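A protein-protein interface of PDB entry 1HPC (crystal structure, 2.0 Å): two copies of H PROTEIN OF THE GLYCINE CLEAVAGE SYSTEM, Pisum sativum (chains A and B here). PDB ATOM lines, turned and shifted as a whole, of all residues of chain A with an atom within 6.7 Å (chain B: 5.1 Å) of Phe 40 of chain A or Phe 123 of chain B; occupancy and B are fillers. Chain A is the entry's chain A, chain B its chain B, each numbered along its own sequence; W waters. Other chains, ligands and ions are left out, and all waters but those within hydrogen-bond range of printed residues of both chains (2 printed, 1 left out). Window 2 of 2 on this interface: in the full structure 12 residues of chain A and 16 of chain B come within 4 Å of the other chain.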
ATOM      1  N   GLU A  37      14.254  24.006  -6.856  1.00  0.00           N
ATOM      2  CA  GLU A  37      13.272  23.849  -5.787  1.00  0.00           C
ATOM      3  C   GLU A  37      13.225  25.046  -4.832  1.00  0.00           C
ATOM      4  O   GLU A  37      14.232  25.368  -4.169  1.00  0.00           O
ATOM      5  CB  GLU A  37      13.599  22.604  -4.988  1.00  0.00           C
ATOM      6  CG  GLU A  37      12.449  22.188  -4.097  1.00  0.00           C
ATOM      7  CD  GLU A  37      12.796  21.504  -2.773  1.00  0.00           C
ATOM      8  OE1 GLU A  37      13.963  21.288  -2.425  1.00  0.00           O
ATOM      9  OE2 GLU A  37      11.842  21.196  -2.068  1.00  0.00           O
ATOM     10  N   VAL A  38      12.048  25.668  -4.730  1.00  0.00           N
ATOM     11  CA  VAL A  38      11.821  26.807  -3.870  1.00  0.00           C
ATOM     12  C   VAL A  38      11.456  26.284  -2.487  1.00  0.00           C
ATOM     13  O   VAL A  38      10.487  25.541  -2.293  1.00  0.00           O
ATOM     14  CB  VAL A  38      10.692  27.661  -4.484  1.00  0.00           C
ATOM     15  CG1 VAL A  38      10.274  28.801  -3.540  1.00  0.00           C
ATOM     16  CG2 VAL A  38      11.224  28.248  -5.804  1.00  0.00           C
ATOM     17  N   VAL A  39      12.277  26.700  -1.517  1.00  0.00           N
ATOM     18  CA  VAL A  39      12.119  26.258  -0.138  1.00  0.00           C
ATOM     19  C   VAL A  39      11.645  27.351   0.817  1.00  0.00           C
ATOM     20  O   VAL A  39      11.269  27.029   1.949  1.00  0.00           O
ATOM     21  CB  VAL A  39      13.471  25.633   0.392  1.00  0.00           C
ATOM     22  CG1 VAL A  39      13.773  24.378  -0.411  1.00  0.00           C
ATOM     23  CG2 VAL A  39      14.633  26.605   0.280  1.00  0.00           C
ATOM     24  N   PHE A  40      11.623  28.644   0.449  1.00  0.00           N
ATOM     25  CA  PHE A  40      11.137  29.685   1.348  1.00  0.00           C
ATOM     26  C   PHE A  40      10.830  30.931   0.535  1.00  0.00           C
ATOM     27  O   PHE A  40      11.420  31.126  -0.528  1.00  0.00           O
ATOM     28  CB  PHE A  40      12.193  30.022   2.399  1.00  0.00           C
ATOM     29  CG  PHE A  40      11.598  30.711   3.632  1.00  0.00           C
ATOM     30  CD1 PHE A  40      10.684  30.017   4.444  1.00  0.00           C
ATOM     31  CD2 PHE A  40      11.957  32.025   3.946  1.00  0.00           C
ATOM     32  CE1 PHE A  40      10.143  30.649   5.567  1.00  0.00           C
ATOM     33  CE2 PHE A  40      11.409  32.640   5.067  1.00  0.00           C
ATOM     34  CZ  PHE A  40      10.507  31.961   5.875  1.00  0.00           C
ATOM     35  N   VAL A  41       9.908  31.785   1.003  1.00  0.00           N
ATOM     36  CA  VAL A  41       9.471  33.001   0.315  1.00  0.00           C
ATOM     37  C   VAL A  41       9.323  34.066   1.391  1.00  0.00           C
ATOM     38  O   VAL A  41       8.816  33.774   2.472  1.00  0.00           O
ATOM     39  CB  VAL A  41       8.060  32.809  -0.401  1.00  0.00           C
ATOM     40  CG1 VAL A  41       7.707  34.043  -1.221  1.00  0.00           C
ATOM     41  CG2 VAL A  41       8.093  31.629  -1.376  1.00  0.00           C
ATOM     42  N   GLU A  42       9.780  35.281   1.137  1.00  0.00           N
ATOM     43  CA  GLU A  42       9.628  36.403   2.054  1.00  0.00           C
ATOM     44  C   GLU A  42       8.737  37.451   1.375  1.00  0.00           C
ATOM     45  O   GLU A  42       9.050  37.901   0.264  1.00  0.00           O
ATOM     46  CB  GLU A  42      10.994  36.992   2.360  1.00  0.00           C
ATOM     47  CG  GLU A  42      11.847  35.979   3.085  1.00  0.00           C
ATOM     48  CD  GLU A  42      13.225  36.535   3.380  1.00  0.00           C
ATOM     49  OE1 GLU A  42      14.109  36.401   2.532  1.00  0.00           O
ATOM     50  OE2 GLU A  42      13.404  37.104   4.453  1.00  0.00           O
ATOM     51  N   ALA A  58      11.516  38.121  -1.553  1.00  0.00           N
ATOM     52  CA  ALA A  58      12.588  37.249  -1.995  1.00  0.00           C
ATOM     53  C   ALA A  58      12.085  35.828  -2.073  1.00  0.00           C
ATOM     54  O   ALA A  58      11.184  35.438  -1.331  1.00  0.00           O
ATOM     55  CB  ALA A  58      13.758  37.239  -1.019  1.00  0.00           C
ATOM     56  N   VAL A  59      12.681  35.061  -2.988  1.00  0.00           N
ATOM     57  CA  VAL A  59      12.372  33.654  -3.161  1.00  0.00           C
ATOM     58  C   VAL A  59      13.693  32.942  -2.880  1.00  0.00           C
ATOM     59  O   VAL A  59      14.737  33.367  -3.364  1.00  0.00           O
ATOM     60  CB  VAL A  59      11.885  33.430  -4.623  1.00  0.00           C
ATOM     61  CG1 VAL A  59      11.576  31.982  -4.860  1.00  0.00           C
ATOM     62  CG2 VAL A  59      10.580  34.171  -4.859  1.00  0.00           C
ATOM     63  N   GLU A  60      13.702  31.895  -2.074  1.00  0.00           N
ATOM     64  CA  GLU A  60      14.918  31.165  -1.775  1.00  0.00           C
ATOM     65  C   GLU A  60      14.768  29.753  -2.276  1.00  0.00           C
ATOM     66  O   GLU A  60      13.773  29.068  -1.989  1.00  0.00           O
ATOM     67  CB  GLU A  60      15.212  31.056  -0.283  1.00  0.00           C
ATOM     68  CG  GLU A  60      15.871  32.288   0.326  1.00  0.00           C
ATOM     69  CD  GLU A  60      14.912  33.271   0.986  1.00  0.00           C
ATOM     70  OE1 GLU A  60      14.196  32.887   1.913  1.00  0.00           O
ATOM     71  OE2 GLU A  60      14.899  34.432   0.584  1.00  0.00           O
ATOM     72  N   SER A  61      15.742  29.326  -3.059  1.00  0.00           N
ATOM     73  CA  SER A  61      15.795  27.974  -3.570  1.00  0.00           C
ATOM     74  C   SER A  61      16.824  27.224  -2.726  1.00  0.00           C
ATOM     75  O   SER A  61      17.430  27.779  -1.789  1.00  0.00           O
ATOM     76  CB  SER A  61      16.226  27.973  -5.049  1.00  0.00           C
ATOM     77  OG  SER A  61      17.619  28.140  -5.322  1.00  0.00           O
ATOM     78  N   LEU A  83       1.837  30.557   0.779  1.00  0.00           N
ATOM     79  CA  LEU A  83       3.205  30.308   0.361  1.00  0.00           C
ATOM     80  C   LEU A  83       4.192  30.094   1.481  1.00  0.00           C
ATOM     81  O   LEU A  83       5.169  29.374   1.279  1.00  0.00           O
ATOM     82  CB  LEU A  83       3.748  31.442  -0.476  1.00  0.00           C
ATOM     83  CG  LEU A  83       3.264  31.599  -1.894  1.00  0.00           C
ATOM     84  CD1 LEU A  83       4.008  32.777  -2.526  1.00  0.00           C
ATOM     85  CD2 LEU A  83       3.545  30.339  -2.693  1.00  0.00           C
ATOM     86  N   THR A  84       3.961  30.663   2.660  1.00  0.00           N
ATOM     87  CA  THR A  84       4.915  30.513   3.748  1.00  0.00           C
ATOM     88  C   THR A  84       5.045  29.054   4.172  1.00  0.00           C
ATOM     89  O   THR A  84       6.133  28.547   4.444  1.00  0.00           O
ATOM     90  CB  THR A  84       4.496  31.359   4.975  1.00  0.00           C
ATOM     91  OG1 THR A  84       3.172  30.947   5.350  1.00  0.00           O
ATOM     92  CG2 THR A  84       4.568  32.852   4.677  1.00  0.00           C
ATOM     93  N   PRO A  87       6.034  26.811   0.068  1.00  0.00           N
ATOM     94  CA  PRO A  87       6.809  27.612  -0.900  1.00  0.00           C
ATOM     95  C   PRO A  87       6.896  26.963  -2.291  1.00  0.00           C
ATOM     96  O   PRO A  87       7.054  27.626  -3.323  1.00  0.00           O
ATOM     97  CB  PRO A  87       8.155  27.762  -0.255  1.00  0.00           C
ATOM     98  CG  PRO A  87       7.976  27.316   1.188  1.00  0.00           C
ATOM     99  CD  PRO A  87       6.915  26.248   1.090  1.00  0.00           C
ATOM    100  N   GLY A  88       6.711  25.636  -2.313  1.00  0.00           N
ATOM    101  CA  GLY A  88       6.745  24.774  -3.493  1.00  0.00           C
ATOM    102  C   GLY A  88       5.673  25.106  -4.521  1.00  0.00           C
ATOM    103  O   GLY A  88       5.844  24.759  -5.690  1.00  0.00           O
ATOM    104  N   ILE A  90       5.288  27.777  -5.899  1.00  0.00           N
ATOM    105  CA  ILE A  90       5.943  28.575  -6.913  1.00  0.00           C
ATOM    106  C   ILE A  90       6.473  27.644  -7.989  1.00  0.00           C
ATOM    107  O   ILE A  90       6.401  28.000  -9.162  1.00  0.00           O
ATOM    108  CB  ILE A  90       7.070  29.416  -6.241  1.00  0.00           C
ATOM    109  CG1 ILE A  90       6.388  30.523  -5.422  1.00  0.00           C
ATOM    110  CG2 ILE A  90       8.019  30.019  -7.272  1.00  0.00           C
ATOM    111  CD1 ILE A  90       7.285  31.613  -4.875  1.00  0.00           C
ATOM    112  N   PRO B  11      16.471  34.199   7.674  1.00  0.00           N
ATOM    113  CA  PRO B  11      16.099  33.083   6.815  1.00  0.00           C
ATOM    114  C   PRO B  11      16.780  33.058   5.450  1.00  0.00           C
ATOM    115  O   PRO B  11      16.943  31.969   4.884  1.00  0.00           O
ATOM    116  CB  PRO B  11      14.586  33.185   6.753  1.00  0.00           C
ATOM    117  CG  PRO B  11      14.285  34.619   7.060  1.00  0.00           C
ATOM    118  CD  PRO B  11      15.294  34.910   8.160  1.00  0.00           C
ATOM    119  N   HIS B  13      19.869  33.374   5.071  1.00  0.00           N
ATOM    120  CA  HIS B  13      21.175  32.799   5.395  1.00  0.00           C
ATOM    121  C   HIS B  13      22.357  33.722   5.558  1.00  0.00           C
ATOM    122  O   HIS B  13      23.510  33.382   5.256  1.00  0.00           O
ATOM    123  CB  HIS B  13      21.554  31.672   4.350  1.00  0.00           C
ATOM    124  CG  HIS B  13      20.491  30.579   4.354  1.00  0.00           C
ATOM    125  ND1 HIS B  13      20.119  29.793   5.359  1.00  0.00           N
ATOM    126  CD2 HIS B  13      19.655  30.310   3.300  1.00  0.00           C
ATOM    127  CE1 HIS B  13      19.101  29.090   4.972  1.00  0.00           C
ATOM    128  NE2 HIS B  13      18.828  29.407   3.731  1.00  0.00           N
ATOM    129  N   LEU B 115      16.488  34.983  13.776  1.00  0.00           N
ATOM    130  CA  LEU B 115      16.540  33.658  14.325  1.00  0.00           C
ATOM    131  C   LEU B 115      17.741  33.469  15.214  1.00  0.00           C
ATOM    132  O   LEU B 115      18.831  33.924  14.874  1.00  0.00           O
ATOM    133  CB  LEU B 115      16.601  32.642  13.197  1.00  0.00           C
ATOM    134  CG  LEU B 115      15.488  32.695  12.152  1.00  0.00           C
ATOM    135  CD1 LEU B 115      15.803  31.733  11.034  1.00  0.00           C
ATOM    136  CD2 LEU B 115      14.156  32.381  12.815  1.00  0.00           C
ATOM    137  N   GLU B 119      17.075  27.871  16.465  1.00  0.00           N
ATOM    138  CA  GLU B 119      16.012  27.949  15.471  1.00  0.00           C
ATOM    139  C   GLU B 119      16.554  27.875  14.060  1.00  0.00           C
ATOM    140  O   GLU B 119      15.970  27.227  13.192  1.00  0.00           O
ATOM    141  CB  GLU B 119      15.207  29.241  15.478  1.00  0.00           C
ATOM    142  CG  GLU B 119      14.386  29.550  16.697  1.00  0.00           C
ATOM    143  CD  GLU B 119      15.013  30.705  17.463  1.00  0.00           C
ATOM    144  OE1 GLU B 119      15.919  30.437  18.268  1.00  0.00           O
ATOM    145  OE2 GLU B 119      14.609  31.858  17.226  1.00  0.00           O
ATOM    146  N   TYR B 120      17.682  28.535  13.834  1.00  0.00           N
ATOM    147  CA  TYR B 120      18.272  28.525  12.525  1.00  0.00           C
ATOM    148  C   TYR B 120      18.683  27.107  12.144  1.00  0.00           C
ATOM    149  O   TYR B 120      18.374  26.675  11.026  1.00  0.00           O
ATOM    150  CB  TYR B 120      19.454  29.464  12.521  1.00  0.00           C
ATOM    151  CG  TYR B 120      20.083  29.560  11.153  1.00  0.00           C
ATOM    152  CD1 TYR B 120      19.359  30.040  10.065  1.00  0.00           C
ATOM    153  CD2 TYR B 120      21.388  29.112  11.009  1.00  0.00           C
ATOM    154  CE1 TYR B 120      19.952  30.055   8.802  1.00  0.00           C
ATOM    155  CE2 TYR B 120      21.979  29.122   9.753  1.00  0.00           C
ATOM    156  CZ  TYR B 120      21.253  29.583   8.650  1.00  0.00           C
ATOM    157  OH  TYR B 120      21.849  29.537   7.392  1.00  0.00           O
ATOM    158  N   THR B 121      19.276  26.346  13.082  1.00  0.00           N
ATOM    159  CA  THR B 121      19.689  24.977  12.798  1.00  0.00           C
ATOM    160  C   THR B 121      18.495  24.139  12.349  1.00  0.00           C
ATOM    161  O   THR B 121      18.587  23.386  11.377  1.00  0.00           O
ATOM    162  CB  THR B 121      20.324  24.336  14.043  1.00  0.00           C
ATOM    163  OG1 THR B 121      21.422  25.147  14.441  1.00  0.00           O
ATOM    164  CG2 THR B 121      20.818  22.930  13.757  1.00  0.00           C
ATOM    165  N   LYS B 122      17.357  24.333  13.022  1.00  0.00           N
ATOM    166  CA  LYS B 122      16.138  23.620  12.687  1.00  0.00           C
ATOM    167  C   LYS B 122      15.596  24.086  11.339  1.00  0.00           C
ATOM    168  O   LYS B 122      15.205  23.259  10.505  1.00  0.00           O
ATOM    169  CB  LYS B 122      15.052  23.847  13.745  1.00  0.00           C
ATOM    170  CG  LYS B 122      15.439  23.801  15.239  1.00  0.00           C
ATOM    171  CD  LYS B 122      16.447  22.702  15.655  1.00  0.00           C
ATOM    172  CE  LYS B 122      17.035  22.933  17.073  1.00  0.00           C
ATOM    173  NZ  LYS B 122      18.485  22.775  17.139  1.00  0.00           N
ATOM    174  N   PHE B 123      15.628  25.392  11.045  1.00  0.00           N
ATOM    175  CA  PHE B 123      15.111  25.940   9.806  1.00  0.00           C
ATOM    176  C   PHE B 123      15.869  25.337   8.634  1.00  0.00           C
ATOM    177  O   PHE B 123      15.277  24.955   7.618  1.00  0.00           O
ATOM    178  CB  PHE B 123      15.247  27.479   9.904  1.00  0.00           C
ATOM    179  CG  PHE B 123      14.959  28.249   8.622  1.00  0.00           C
ATOM    180  CD1 PHE B 123      13.654  28.607   8.287  1.00  0.00           C
ATOM    181  CD2 PHE B 123      16.020  28.561   7.764  1.00  0.00           C
ATOM    182  CE1 PHE B 123      13.413  29.284   7.085  1.00  0.00           C
ATOM    183  CE2 PHE B 123      15.771  29.234   6.572  1.00  0.00           C
ATOM    184  CZ  PHE B 123      14.468  29.590   6.233  1.00  0.00           C
ATOM    185  N   CYS B 124      17.182  25.187   8.777  1.00  0.00           N
ATOM    186  CA  CYS B 124      18.004  24.602   7.741  1.00  0.00           C
ATOM    187  C   CYS B 124      17.673  23.147   7.439  1.00  0.00           C
ATOM    188  O   CYS B 124      17.814  22.706   6.283  1.00  0.00           O
ATOM    189  CB  CYS B 124      19.455  24.734   8.145  1.00  0.00           C
ATOM    190  SG  CYS B 124      19.976  26.463   7.958  1.00  0.00           S
ATOM    191  N   GLU B 125      17.196  22.436   8.466  1.00  0.00           N
ATOM    192  CA  GLU B 125      16.760  21.044   8.392  1.00  0.00           C
ATOM    193  C   GLU B 125      15.480  20.868   7.624  1.00  0.00           C
ATOM    194  O   GLU B 125      15.383  19.930   6.832  1.00  0.00           O
ATOM    195  CB  GLU B 125      16.540  20.462   9.773  1.00  0.00           C
ATOM    196  CG  GLU B 125      17.887  20.204  10.412  1.00  0.00           C
ATOM    197  CD  GLU B 125      17.891  19.781  11.877  1.00  0.00           C
ATOM    198  OE1 GLU B 125      16.845  19.413  12.433  1.00  0.00           O
ATOM    199  OE2 GLU B 125      18.977  19.824  12.460  1.00  0.00           O
ATOM    200  N   GLU B 126      14.481  21.722   7.857  1.00  0.00           N
ATOM    201  CA  GLU B 126      13.272  21.689   7.050  1.00  0.00           C
ATOM    202  C   GLU B 126      13.724  21.903   5.614  1.00  0.00           C
ATOM    203  O   GLU B 126      13.450  21.056   4.768  1.00  0.00           O
ATOM    204  CB  GLU B 126      12.252  22.814   7.407  1.00  0.00           C
ATOM    205  CG  GLU B 126      11.045  23.099   6.430  1.00  0.00           C
ATOM    206  CD  GLU B 126      11.119  24.341   5.493  1.00  0.00           C
ATOM    207  OE1 GLU B 126      11.120  25.483   5.993  1.00  0.00           O
ATOM    208  OE2 GLU B 126      11.140  24.166   4.258  1.00  0.00           O
ATOM    209  N   GLU B 127      14.490  22.969   5.347  1.00  0.00           N
ATOM    210  CA  GLU B 127      14.870  23.282   3.986  1.00  0.00           C
ATOM    211  C   GLU B 127      15.518  22.160   3.199  1.00  0.00           C
ATOM    212  O   GLU B 127      15.149  21.911   2.045  1.00  0.00           O
ATOM    213  CB  GLU B 127      15.810  24.452   3.976  1.00  0.00           C
ATOM    214  CG  GLU B 127      15.054  25.697   4.393  1.00  0.00           C
ATOM    215  CD  GLU B 127      15.692  26.972   3.864  1.00  0.00           C
ATOM    216  OE1 GLU B 127      16.926  27.054   3.787  1.00  0.00           O
ATOM    217  OE2 GLU B 127      14.933  27.882   3.520  1.00  0.00           O
HETATM  218  O   HOH W   1       8.472  26.397   4.953  1.00  0.00           O
HETATM  219  O   HOH W   2      18.169  28.975   0.640  1.00  0.00           O
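The backbone carbonyl oxygen (O) of Ala 58 of chain A is in hydrogen-bond range of the backbone NH (N) of Glu 42 of chain A (2.8 Å).
NE2 of His 13 of chain B lies within hydrogen-bond range of OE1 of Glu 127 of chain B (3.0 Å).
O of Pro 11 of chain B sits at hydrogen-bond distance from NE2 of His 13 of chain B.
The backbone carbonyl oxygen of Phe 40 of chain A sits at hydrogen-bond distance from the backbone NH of Glu 60 of chain A (2.9 Å).
N of Val 39 of chain A sits at hydrogen-bond distance from O of Glu 60 of chain A (2.8 Å).
Among the printed residues, merely in contact across the chains: Val 39 of chain A with Glu 127 of chain B (3.5 Å), Phe 40 of chain A with Pro 11 of chain B (3.6 Å), Phe 40 of chain A with Glu 127 of chain B (3.7 Å), Val 39 of chain A with Glu 126 of chain B (3.7 Å), Glu 42 of chain A with Pro 11 of chain B (3.7 Å) and Phe 40 of chain A with Phe 123 of chain B (3.9 Å).
Printed residues of chain A within 4 Å of Phe 123 of chain B: Phe 40.
Of the printed residues of chain A, Pro 11 of chain B touches Phe 40 (3.6 Å) and Glu 42 (3.7 Å).
Of the printed residues of chain A, Glu 127 of chain B touches Val 39 and Phe 40.
Printed residues of chain B within 4 Å of Val 39 of chain A: Glu 126 (3.7 Å) and Glu 127 (3.5 Å).
Printed residues of chain B within 4 Å of Glu 42 of chain A: Pro 11.
Printed residues of chain A within 4 Å of Glu 126 of chain B: Val 39 (3.7 Å).
Leu 83 of chain A touches none of the printed residues of chain B.
The nearest residue of chain A that does not touch Phe 123 of chain B is Glu 60 of chain A (5.4 Å).
The nearest printed residue of chain A that does not touch Glu 127 of chain B is Glu 37 of chain A (4.7 Å).
Printed residues of chain B that touch a printed residue of chain A: Pro 11, Phe 123, Glu 126 and Glu 127.
Hydrophobic or aromatic side chains of chain B that line the printed part of chain A: Pro 11 and Phe 123.
Of the 15 printed residues of chain A, 3 touch a printed residue of chain B.
Printed residues of chain A that touch a printed residue of chain B: Val 39, Phe 40 and Glu 42.
Hydrophobic or aromatic side chains of chain A that line the printed part of chain B: Val 39 and Phe 40.
Among the printed residues, no Asp or Glu carboxylate lies within 4 Å of a Lys or Arg side-chain nitrogen of the other chain.
No position is printed for both chains.
Water W2 bridges the backbone carbonyl oxygen of Ser 61 of chain A (2.8 Å) and a ring nitrogen (NE2) of His 13 of chain B (3.2 Å).
Water W1 lies within hydrogen-bond range of OE1 of Glu 126 of chain B (3.0 Å) and O of Thr 84 of chain A (3.2 Å).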
